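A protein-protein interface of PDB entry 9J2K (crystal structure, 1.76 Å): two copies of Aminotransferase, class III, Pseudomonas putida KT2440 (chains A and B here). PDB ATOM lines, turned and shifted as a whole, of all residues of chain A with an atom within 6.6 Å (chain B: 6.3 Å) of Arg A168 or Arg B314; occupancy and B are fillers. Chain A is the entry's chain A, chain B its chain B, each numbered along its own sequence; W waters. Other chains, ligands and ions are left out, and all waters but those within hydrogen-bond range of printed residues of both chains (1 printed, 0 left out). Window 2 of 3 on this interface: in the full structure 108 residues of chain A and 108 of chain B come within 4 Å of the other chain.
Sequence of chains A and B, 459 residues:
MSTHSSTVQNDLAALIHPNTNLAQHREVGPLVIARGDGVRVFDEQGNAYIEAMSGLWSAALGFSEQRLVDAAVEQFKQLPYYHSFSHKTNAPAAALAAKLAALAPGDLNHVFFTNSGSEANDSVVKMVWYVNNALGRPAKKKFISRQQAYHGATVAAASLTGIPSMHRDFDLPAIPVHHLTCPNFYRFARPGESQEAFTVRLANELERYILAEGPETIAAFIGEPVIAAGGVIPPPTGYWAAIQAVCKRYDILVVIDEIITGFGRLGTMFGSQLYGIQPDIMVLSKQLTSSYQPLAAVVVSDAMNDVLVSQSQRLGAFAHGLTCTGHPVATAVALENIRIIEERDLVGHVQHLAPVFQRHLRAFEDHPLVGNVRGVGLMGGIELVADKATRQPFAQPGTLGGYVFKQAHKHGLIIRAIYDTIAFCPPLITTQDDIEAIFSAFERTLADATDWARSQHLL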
ATOM      1  N   ALA A  23      -6.648  39.844 -11.918  1.00  0.00           N
ATOM      2  CA  ALA A  23      -5.548  40.408 -11.141  1.00  0.00           C
ATOM      3  C   ALA A  23      -5.018  41.677 -11.784  1.00  0.00           C
ATOM      4  O   ALA A  23      -4.837  42.700 -11.110  1.00  0.00           O
ATOM      5  CB  ALA A  23      -4.424  39.396 -11.005  1.00  0.00           C
ATOM      6  N   ILE A 163     -11.846  25.093 -26.579  1.00  0.00           N
ATOM      7  CA  ILE A 163     -10.681  25.936 -26.293  1.00  0.00           C
ATOM      8  C   ILE A 163     -10.139  25.562 -24.916  1.00  0.00           C
ATOM      9  O   ILE A 163     -10.835  25.753 -23.913  1.00  0.00           O
ATOM     10  CB  ILE A 163     -11.051  27.427 -26.369  1.00  0.00           C
ATOM     11  CG1 ILE A 163     -11.525  27.757 -27.783  1.00  0.00           C
ATOM     12  CG2 ILE A 163      -9.863  28.307 -25.955  1.00  0.00           C
ATOM     13  CD1 ILE A 163     -12.324  29.031 -27.886  1.00  0.00           C
ATOM     14  N   PRO A 164      -8.913  25.033 -24.817  1.00  0.00           N
ATOM     15  CA  PRO A 164      -8.481  24.421 -23.545  1.00  0.00           C
ATOM     16  C   PRO A 164      -8.469  25.376 -22.362  1.00  0.00           C
ATOM     17  O   PRO A 164      -8.752  24.946 -21.236  1.00  0.00           O
ATOM     18  CB  PRO A 164      -7.068  23.905 -23.863  1.00  0.00           C
ATOM     19  CG  PRO A 164      -7.051  23.737 -25.350  1.00  0.00           C
ATOM     20  CD  PRO A 164      -7.926  24.838 -25.894  1.00  0.00           C
ATOM     21  N   SER A 165      -8.162  26.661 -22.571  1.00  0.00           N
ATOM     22  CA  SER A 165      -8.144  27.594 -21.450  1.00  0.00           C
ATOM     23  C   SER A 165      -9.524  27.777 -20.834  1.00  0.00           C
ATOM     24  O   SER A 165      -9.626  28.154 -19.661  1.00  0.00           O
ATOM     25  CB  SER A 165      -7.584  28.949 -21.904  1.00  0.00           C
ATOM     26  OG  SER A 165      -8.364  29.500 -22.954  1.00  0.00           O
ATOM     27  N   MET A 166     -10.585  27.509 -21.592  1.00  0.00           N
ATOM     28  CA  MET A 166     -11.922  27.612 -21.033  1.00  0.00           C
ATOM     29  C   MET A 166     -12.321  26.375 -20.236  1.00  0.00           C
ATOM     30  O   MET A 166     -13.343  26.413 -19.541  1.00  0.00           O
ATOM     31  CB  MET A 166     -12.917  27.888 -22.156  1.00  0.00           C
ATOM     32  CG  MET A 166     -12.354  28.885 -23.154  1.00  0.00           C
ATOM     33  SD  MET A 166     -13.606  29.698 -24.141  1.00  0.00           S
ATOM     34  CE  MET A 166     -14.258  30.856 -22.941  1.00  0.00           C
ATOM     35  N   HIS A 167     -11.524  25.304 -20.283  1.00  0.00           N
ATOM     36  CA  HIS A 167     -11.767  24.140 -19.439  1.00  0.00           C
ATOM     37  C   HIS A 167     -10.923  24.133 -18.179  1.00  0.00           C
ATOM     38  O   HIS A 167     -11.299  23.471 -17.202  1.00  0.00           O
ATOM     39  CB  HIS A 167     -11.469  22.848 -20.206  1.00  0.00           C
ATOM     40  CG  HIS A 167     -12.405  22.594 -21.343  1.00  0.00           C
ATOM     41  ND1 HIS A 167     -12.119  21.709 -22.363  1.00  0.00           N
ATOM     42  CD2 HIS A 167     -13.632  23.099 -21.615  1.00  0.00           C
ATOM     43  CE1 HIS A 167     -13.121  21.698 -23.226  1.00  0.00           C
ATOM     44  NE2 HIS A 167     -14.054  22.527 -22.793  1.00  0.00           N
ATOM     45  N   ARG A 168      -9.798  24.840 -18.186  1.00  0.00           N
ATOM     46  CA  ARG A 168      -8.799  24.665 -17.146  1.00  0.00           C
ATOM     47  C   ARG A 168      -9.335  25.098 -15.788  1.00  0.00           C
ATOM     48  O   ARG A 168      -9.803  26.231 -15.621  1.00  0.00           O
ATOM     49  CB  ARG A 168      -7.541  25.445 -17.507  1.00  0.00           C
ATOM     50  CG  ARG A 168      -6.375  25.103 -16.616  1.00  0.00           C
ATOM     51  CD  ARG A 168      -5.081  25.633 -17.191  1.00  0.00           C
ATOM     52  NE  ARG A 168      -3.956  25.275 -16.339  1.00  0.00           N
ATOM     53  CZ  ARG A 168      -2.728  25.752 -16.477  1.00  0.00           C
ATOM     54  NH1 ARG A 168      -2.426  26.613 -17.433  1.00  0.00           N
ATOM     55  NH2 ARG A 168      -1.782  25.357 -15.631  1.00  0.00           N
ATOM     56  N   ASP A 169      -9.258  24.177 -14.823  1.00  0.00           N
ATOM     57  CA  ASP A 169      -9.713  24.324 -13.440  1.00  0.00           C
ATOM     58  C   ASP A 169     -11.223  24.467 -13.319  1.00  0.00           C
ATOM     59  O   ASP A 169     -11.715  24.719 -12.214  1.00  0.00           O
ATOM     60  CB  ASP A 169      -9.032  25.491 -12.709  1.00  0.00           C
ATOM     61  CG  ASP A 169      -7.604  25.170 -12.316  1.00  0.00           C
ATOM     62  OD1 ASP A 169      -7.148  24.059 -12.642  1.00  0.00           O
ATOM     63  OD2 ASP A 169      -6.936  26.022 -11.698  1.00  0.00           O
ATOM     64  N   PHE A 170     -11.979  24.280 -14.406  1.00  0.00           N
ATOM     65  CA  PHE A 170     -13.436  24.246 -14.318  1.00  0.00           C
ATOM     66  C   PHE A 170     -13.995  22.830 -14.349  1.00  0.00           C
ATOM     67  O   PHE A 170     -15.219  22.665 -14.416  1.00  0.00           O
ATOM     68  CB  PHE A 170     -14.070  25.061 -15.458  1.00  0.00           C
ATOM     69  CG  PHE A 170     -13.987  26.566 -15.270  1.00  0.00           C
ATOM     70  CD1 PHE A 170     -14.577  27.173 -14.168  1.00  0.00           C
ATOM     71  CD2 PHE A 170     -13.350  27.369 -16.211  1.00  0.00           C
ATOM     72  CE1 PHE A 170     -14.521  28.552 -13.992  1.00  0.00           C
ATOM     73  CE2 PHE A 170     -13.287  28.747 -16.046  1.00  0.00           C
ATOM     74  CZ  PHE A 170     -13.869  29.346 -14.937  1.00  0.00           C
ATOM     75  N   ASP A 171     -13.131  21.807 -14.335  1.00  0.00           N
ATOM     76  CA  ASP A 171     -13.565  20.403 -14.375  1.00  0.00           C
ATOM     77  C   ASP A 171     -14.419  20.124 -15.609  1.00  0.00           C
ATOM     78  O   ASP A 171     -15.441  19.436 -15.535  1.00  0.00           O
ATOM     79  CB  ASP A 171     -14.326  20.005 -13.103  1.00  0.00           C
ATOM     80  CG  ASP A 171     -13.455  20.025 -11.863  1.00  0.00           C
ATOM     81  OD1 ASP A 171     -12.225  20.210 -11.973  1.00  0.00           O
ATOM     82  OD2 ASP A 171     -14.015  19.825 -10.768  1.00  0.00           O
ATOM     83  N   LEU A 172     -14.008  20.671 -16.745  1.00  0.00           N
ATOM     84  CA  LEU A 172     -14.725  20.474 -17.995  1.00  0.00           C
ATOM     85  C   LEU A 172     -13.869  19.673 -18.960  1.00  0.00           C
ATOM     86  O   LEU A 172     -12.639  19.719 -18.870  1.00  0.00           O
ATOM     87  CB  LEU A 172     -15.090  21.813 -18.645  1.00  0.00           C
ATOM     88  CG  LEU A 172     -15.934  22.726 -17.755  1.00  0.00           C
ATOM     89  CD1 LEU A 172     -16.110  24.087 -18.434  1.00  0.00           C
ATOM     90  CD2 LEU A 172     -17.276  22.082 -17.451  1.00  0.00           C
ATOM     91  N   TYR B 130     -13.838  25.893  -9.604  1.00  0.00           N
ATOM     92  CA  TYR B 130     -12.624  26.664  -9.872  1.00  0.00           C
ATOM     93  C   TYR B 130     -11.902  27.038  -8.579  1.00  0.00           C
ATOM     94  O   TYR B 130     -10.688  26.833  -8.444  1.00  0.00           O
ATOM     95  CB  TYR B 130     -13.059  27.895 -10.650  1.00  0.00           C
ATOM     96  CG  TYR B 130     -12.085  28.796 -11.353  1.00  0.00           C
ATOM     97  CD1 TYR B 130     -11.455  28.412 -12.532  1.00  0.00           C
ATOM     98  CD2 TYR B 130     -11.923  30.103 -10.918  1.00  0.00           C
ATOM     99  CE1 TYR B 130     -10.623  29.294 -13.217  1.00  0.00           C
ATOM    100  CE2 TYR B 130     -11.105  30.988 -11.595  1.00  0.00           C
ATOM    101  CZ  TYR B 130     -10.459  30.586 -12.739  1.00  0.00           C
ATOM    102  OH  TYR B 130      -9.658  31.488 -13.398  1.00  0.00           O
ATOM    103  N   ASN B 133     -10.358  23.937  -6.942  1.00  0.00           N
ATOM    104  CA  ASN B 133      -9.117  23.566  -7.615  1.00  0.00           C
ATOM    105  C   ASN B 133      -7.995  24.525  -7.248  1.00  0.00           C
ATOM    106  O   ASN B 133      -6.865  24.094  -6.976  1.00  0.00           O
ATOM    107  CB  ASN B 133      -9.317  23.515  -9.134  1.00  0.00           C
ATOM    108  CG  ASN B 133     -10.105  22.296  -9.572  1.00  0.00           C
ATOM    109  OD1 ASN B 133      -9.921  21.198  -9.034  1.00  0.00           O
ATOM    110  ND2 ASN B 133     -11.000  22.476 -10.537  1.00  0.00           N
ATOM    111  N   ALA B 134      -8.290  25.828  -7.222  1.00  0.00           N
ATOM    112  CA  ALA B 134      -7.271  26.820  -6.887  1.00  0.00           C
ATOM    113  C   ALA B 134      -6.694  26.581  -5.497  1.00  0.00           C
ATOM    114  O   ALA B 134      -5.504  26.815  -5.257  1.00  0.00           O
ATOM    115  CB  ALA B 134      -7.864  28.223  -6.959  1.00  0.00           C
ATOM    116  N   VAL B 309      -9.218  36.055  -8.127  1.00  0.00           N
ATOM    117  CA  VAL B 309      -8.125  36.928  -8.534  1.00  0.00           C
ATOM    118  C   VAL B 309      -6.797  36.170  -8.538  1.00  0.00           C
ATOM    119  O   VAL B 309      -5.974  36.344  -9.446  1.00  0.00           O
ATOM    120  CB  VAL B 309      -8.078  38.167  -7.620  1.00  0.00           C
ATOM    121  CG1 VAL B 309      -6.778  38.946  -7.841  1.00  0.00           C
ATOM    122  CG2 VAL B 309      -9.312  39.044  -7.862  1.00  0.00           C
ATOM    123  N   SER B 310      -6.569  35.307  -7.540  1.00  0.00           N
ATOM    124  CA  SER B 310      -5.327  34.534  -7.535  1.00  0.00           C
ATOM    125  C   SER B 310      -5.246  33.588  -8.736  1.00  0.00           C
ATOM    126  O   SER B 310      -4.147  33.265  -9.200  1.00  0.00           O
ATOM    127  CB  SER B 310      -5.185  33.759  -6.218  1.00  0.00           C
ATOM    128  OG  SER B 310      -6.098  32.677  -6.126  1.00  0.00           O
ATOM    129  N   GLN B 311      -6.396  33.168  -9.272  1.00  0.00           N
ATOM    130  CA  GLN B 311      -6.409  32.289 -10.441  1.00  0.00           C
ATOM    131  C   GLN B 311      -6.024  33.039 -11.709  1.00  0.00           C
ATOM    132  O   GLN B 311      -5.270  32.517 -12.540  1.00  0.00           O
ATOM    133  CB  GLN B 311      -7.791  31.659 -10.615  1.00  0.00           C
ATOM    134  CG  GLN B 311      -8.080  30.528  -9.648  1.00  0.00           C
ATOM    135  CD  GLN B 311      -7.355  29.267 -10.048  1.00  0.00           C
ATOM    136  OE1 GLN B 311      -6.141  29.147  -9.857  1.00  0.00           O
ATOM    137  NE2 GLN B 311      -8.088  28.320 -10.619  1.00  0.00           N
ATOM    138  N   SER B 312      -6.578  34.239 -11.902  1.00  0.00           N
ATOM    139  CA  SER B 312      -6.183  35.039 -13.057  1.00  0.00           C
ATOM    140  C   SER B 312      -4.683  35.299 -13.044  1.00  0.00           C
ATOM    141  O   SER B 312      -4.042  35.324 -14.104  1.00  0.00           O
ATOM    142  CB  SER B 312      -6.965  36.351 -13.092  1.00  0.00           C
ATOM    143  OG  SER B 312      -8.209  36.182 -13.758  1.00  0.00           O
ATOM    144  N   GLN B 313      -4.106  35.478 -11.851  1.00  0.00           N
ATOM    145  CA  GLN B 313      -2.667  35.679 -11.744  1.00  0.00           C
ATOM    146  C   GLN B 313      -1.897  34.528 -12.389  1.00  0.00           C
ATOM    147  O   GLN B 313      -0.905  34.755 -13.089  1.00  0.00           O
ATOM    148  CB  GLN B 313      -2.275  35.848 -10.276  1.00  0.00           C
ATOM    149  CG  GLN B 313      -0.792  36.102 -10.060  1.00  0.00           C
ATOM    150  CD  GLN B 313      -0.338  37.416 -10.653  1.00  0.00           C
ATOM    151  OE1 GLN B 313      -0.843  38.482 -10.296  1.00  0.00           O
ATOM    152  NE2 GLN B 313       0.621  37.347 -11.567  1.00  0.00           N
ATOM    153  N   ARG B 314      -2.339  33.285 -12.172  1.00  0.00           N
ATOM    154  CA  ARG B 314      -1.610  32.138 -12.711  1.00  0.00           C
ATOM    155  C   ARG B 314      -2.153  31.619 -14.040  1.00  0.00           C
ATOM    156  O   ARG B 314      -1.393  31.019 -14.806  1.00  0.00           O
ATOM    157  CB  ARG B 314      -1.586  30.980 -11.698  1.00  0.00           C
ATOM    158  CG  ARG B 314      -2.931  30.556 -11.125  1.00  0.00           C
ATOM    159  CD  ARG B 314      -2.796  29.326 -10.203  1.00  0.00           C
ATOM    160  NE  ARG B 314      -2.344  28.131 -10.912  1.00  0.00           N
ATOM    161  CZ  ARG B 314      -3.142  27.160 -11.343  1.00  0.00           C
ATOM    162  NH1 ARG B 314      -4.450  27.195 -11.136  1.00  0.00           N
ATOM    163  NH2 ARG B 314      -2.613  26.125 -11.991  1.00  0.00           N
ATOM    164  N   LEU B 315      -3.434  31.839 -14.346  1.00  0.00           N
ATOM    165  CA  LEU B 315      -4.026  31.331 -15.578  1.00  0.00           C
ATOM    166  C   LEU B 315      -4.137  32.376 -16.680  1.00  0.00           C
ATOM    167  O   LEU B 315      -4.266  32.002 -17.847  1.00  0.00           O
ATOM    168  CB  LEU B 315      -5.424  30.761 -15.304  1.00  0.00           C
ATOM    169  CG  LEU B 315      -5.476  29.584 -14.325  1.00  0.00           C
ATOM    170  CD1 LEU B 315      -6.912  29.125 -14.103  1.00  0.00           C
ATOM    171  CD2 LEU B 315      -4.593  28.425 -14.803  1.00  0.00           C
ATOM    172  N   GLY B 316      -4.107  33.661 -16.347  1.00  0.00           N
ATOM    173  CA  GLY B 316      -4.117  34.713 -17.339  1.00  0.00           C
ATOM    174  C   GLY B 316      -5.451  35.411 -17.534  1.00  0.00           C
ATOM    175  O   GLY B 316      -5.473  36.538 -18.047  1.00  0.00           O
ATOM    176  N   ALA B 317      -6.554  34.780 -17.146  1.00  0.00           N
ATOM    177  CA  ALA B 317      -7.884  35.346 -17.337  1.00  0.00           C
ATOM    178  C   ALA B 317      -8.881  34.504 -16.560  1.00  0.00           C
ATOM    179  O   ALA B 317      -8.639  33.329 -16.280  1.00  0.00           O
ATOM    180  CB  ALA B 317      -8.283  35.392 -18.816  1.00  0.00           C
HETATM  181  O   HOH W   1      -4.452  24.190 -13.378  1.00  0.00           O
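The side-chain carboxylate (OD2) of Asp A169 is in salt-bridge range of the guanidinium group (NH1) of Arg B314, at 2.8 Å.
OD1 of Asp A171 is in hydrogen-bond range of ND2 of Asn B133 (2.9 Å).
O of Asp A169 sits at hydrogen-bond distance from ND2 of Asn B133, at 2.9 Å.
OD2 of Asp A169 is in hydrogen-bond range of NE2 of Gln B311 (2.8 Å).
The guanidinium group (NH1) of Arg B314 sits at hydrogen-bond distance from the side-chain amide oxygen (OE1) of Gln B311 (2.9 Å).
Val B309 touches Ala A23.
N of Ala A23 touches CB of Ser B312, 3.7 Å away.
Ala A23 touches Gln B313.
O of Arg A168 touches CE1 of Tyr B130, 3.98 Å away.
NH2 of Arg A168 touches NH2 of Arg B314, 3.8 Å away.
Arg A168 touches Leu B315.
Asp A169 touches Tyr B130.
OD2 of Asp A169 touches CD1 of Leu B315 (3.9 Å).
CE1 of Phe A170 touches CD1 of Tyr B130 (3.4 Å).
Of chain B, only Tyr B130 (3.98 Å), Arg B314 (3.8 Å) and Leu B315 (3.6 Å) come within 4 Å of Arg A168.
Arg B314 touches just these residues of chain A: Arg A168 (3.8 Å) and Asp A169 (2.8 Å).
Of the printed residues of chain A, Tyr B130 touches Arg A168, Asp A169 and Phe A170.
Printed residues of chain A within 4 Å of Val B309: Ala A23 (3.8 Å).
Met A166 touches none of the printed residues of chain B.
The nearest residue of chain B that does not touch Arg A168 is Gln B311 (5.7 Å).
Of the 11 printed residues of chain A, 5 touch a printed residue of chain B.
Hydrophobic or aromatic side chains of chain A within 4 Å of the printed part of chain B: Ala A23 and Phe A170.
Hydrophobic or aromatic side chains of chain B within 4 Å of the printed part of chain A: Tyr B130, Val B309 and Leu B315.
Among the printed residues, Asp or Glu carboxylates within 4 Å of a Lys or Arg side-chain nitrogen of the other chain: Asp A169 with Arg B314.
No position is printed for both chains.
Water W1 lies within hydrogen-bond range of the side-chain carboxylate of Asp A169 (2.8 Å), the guanidinium group of Arg B314 (3.0 Å) and the guanidinium group of Arg A168 (3.2 Å).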
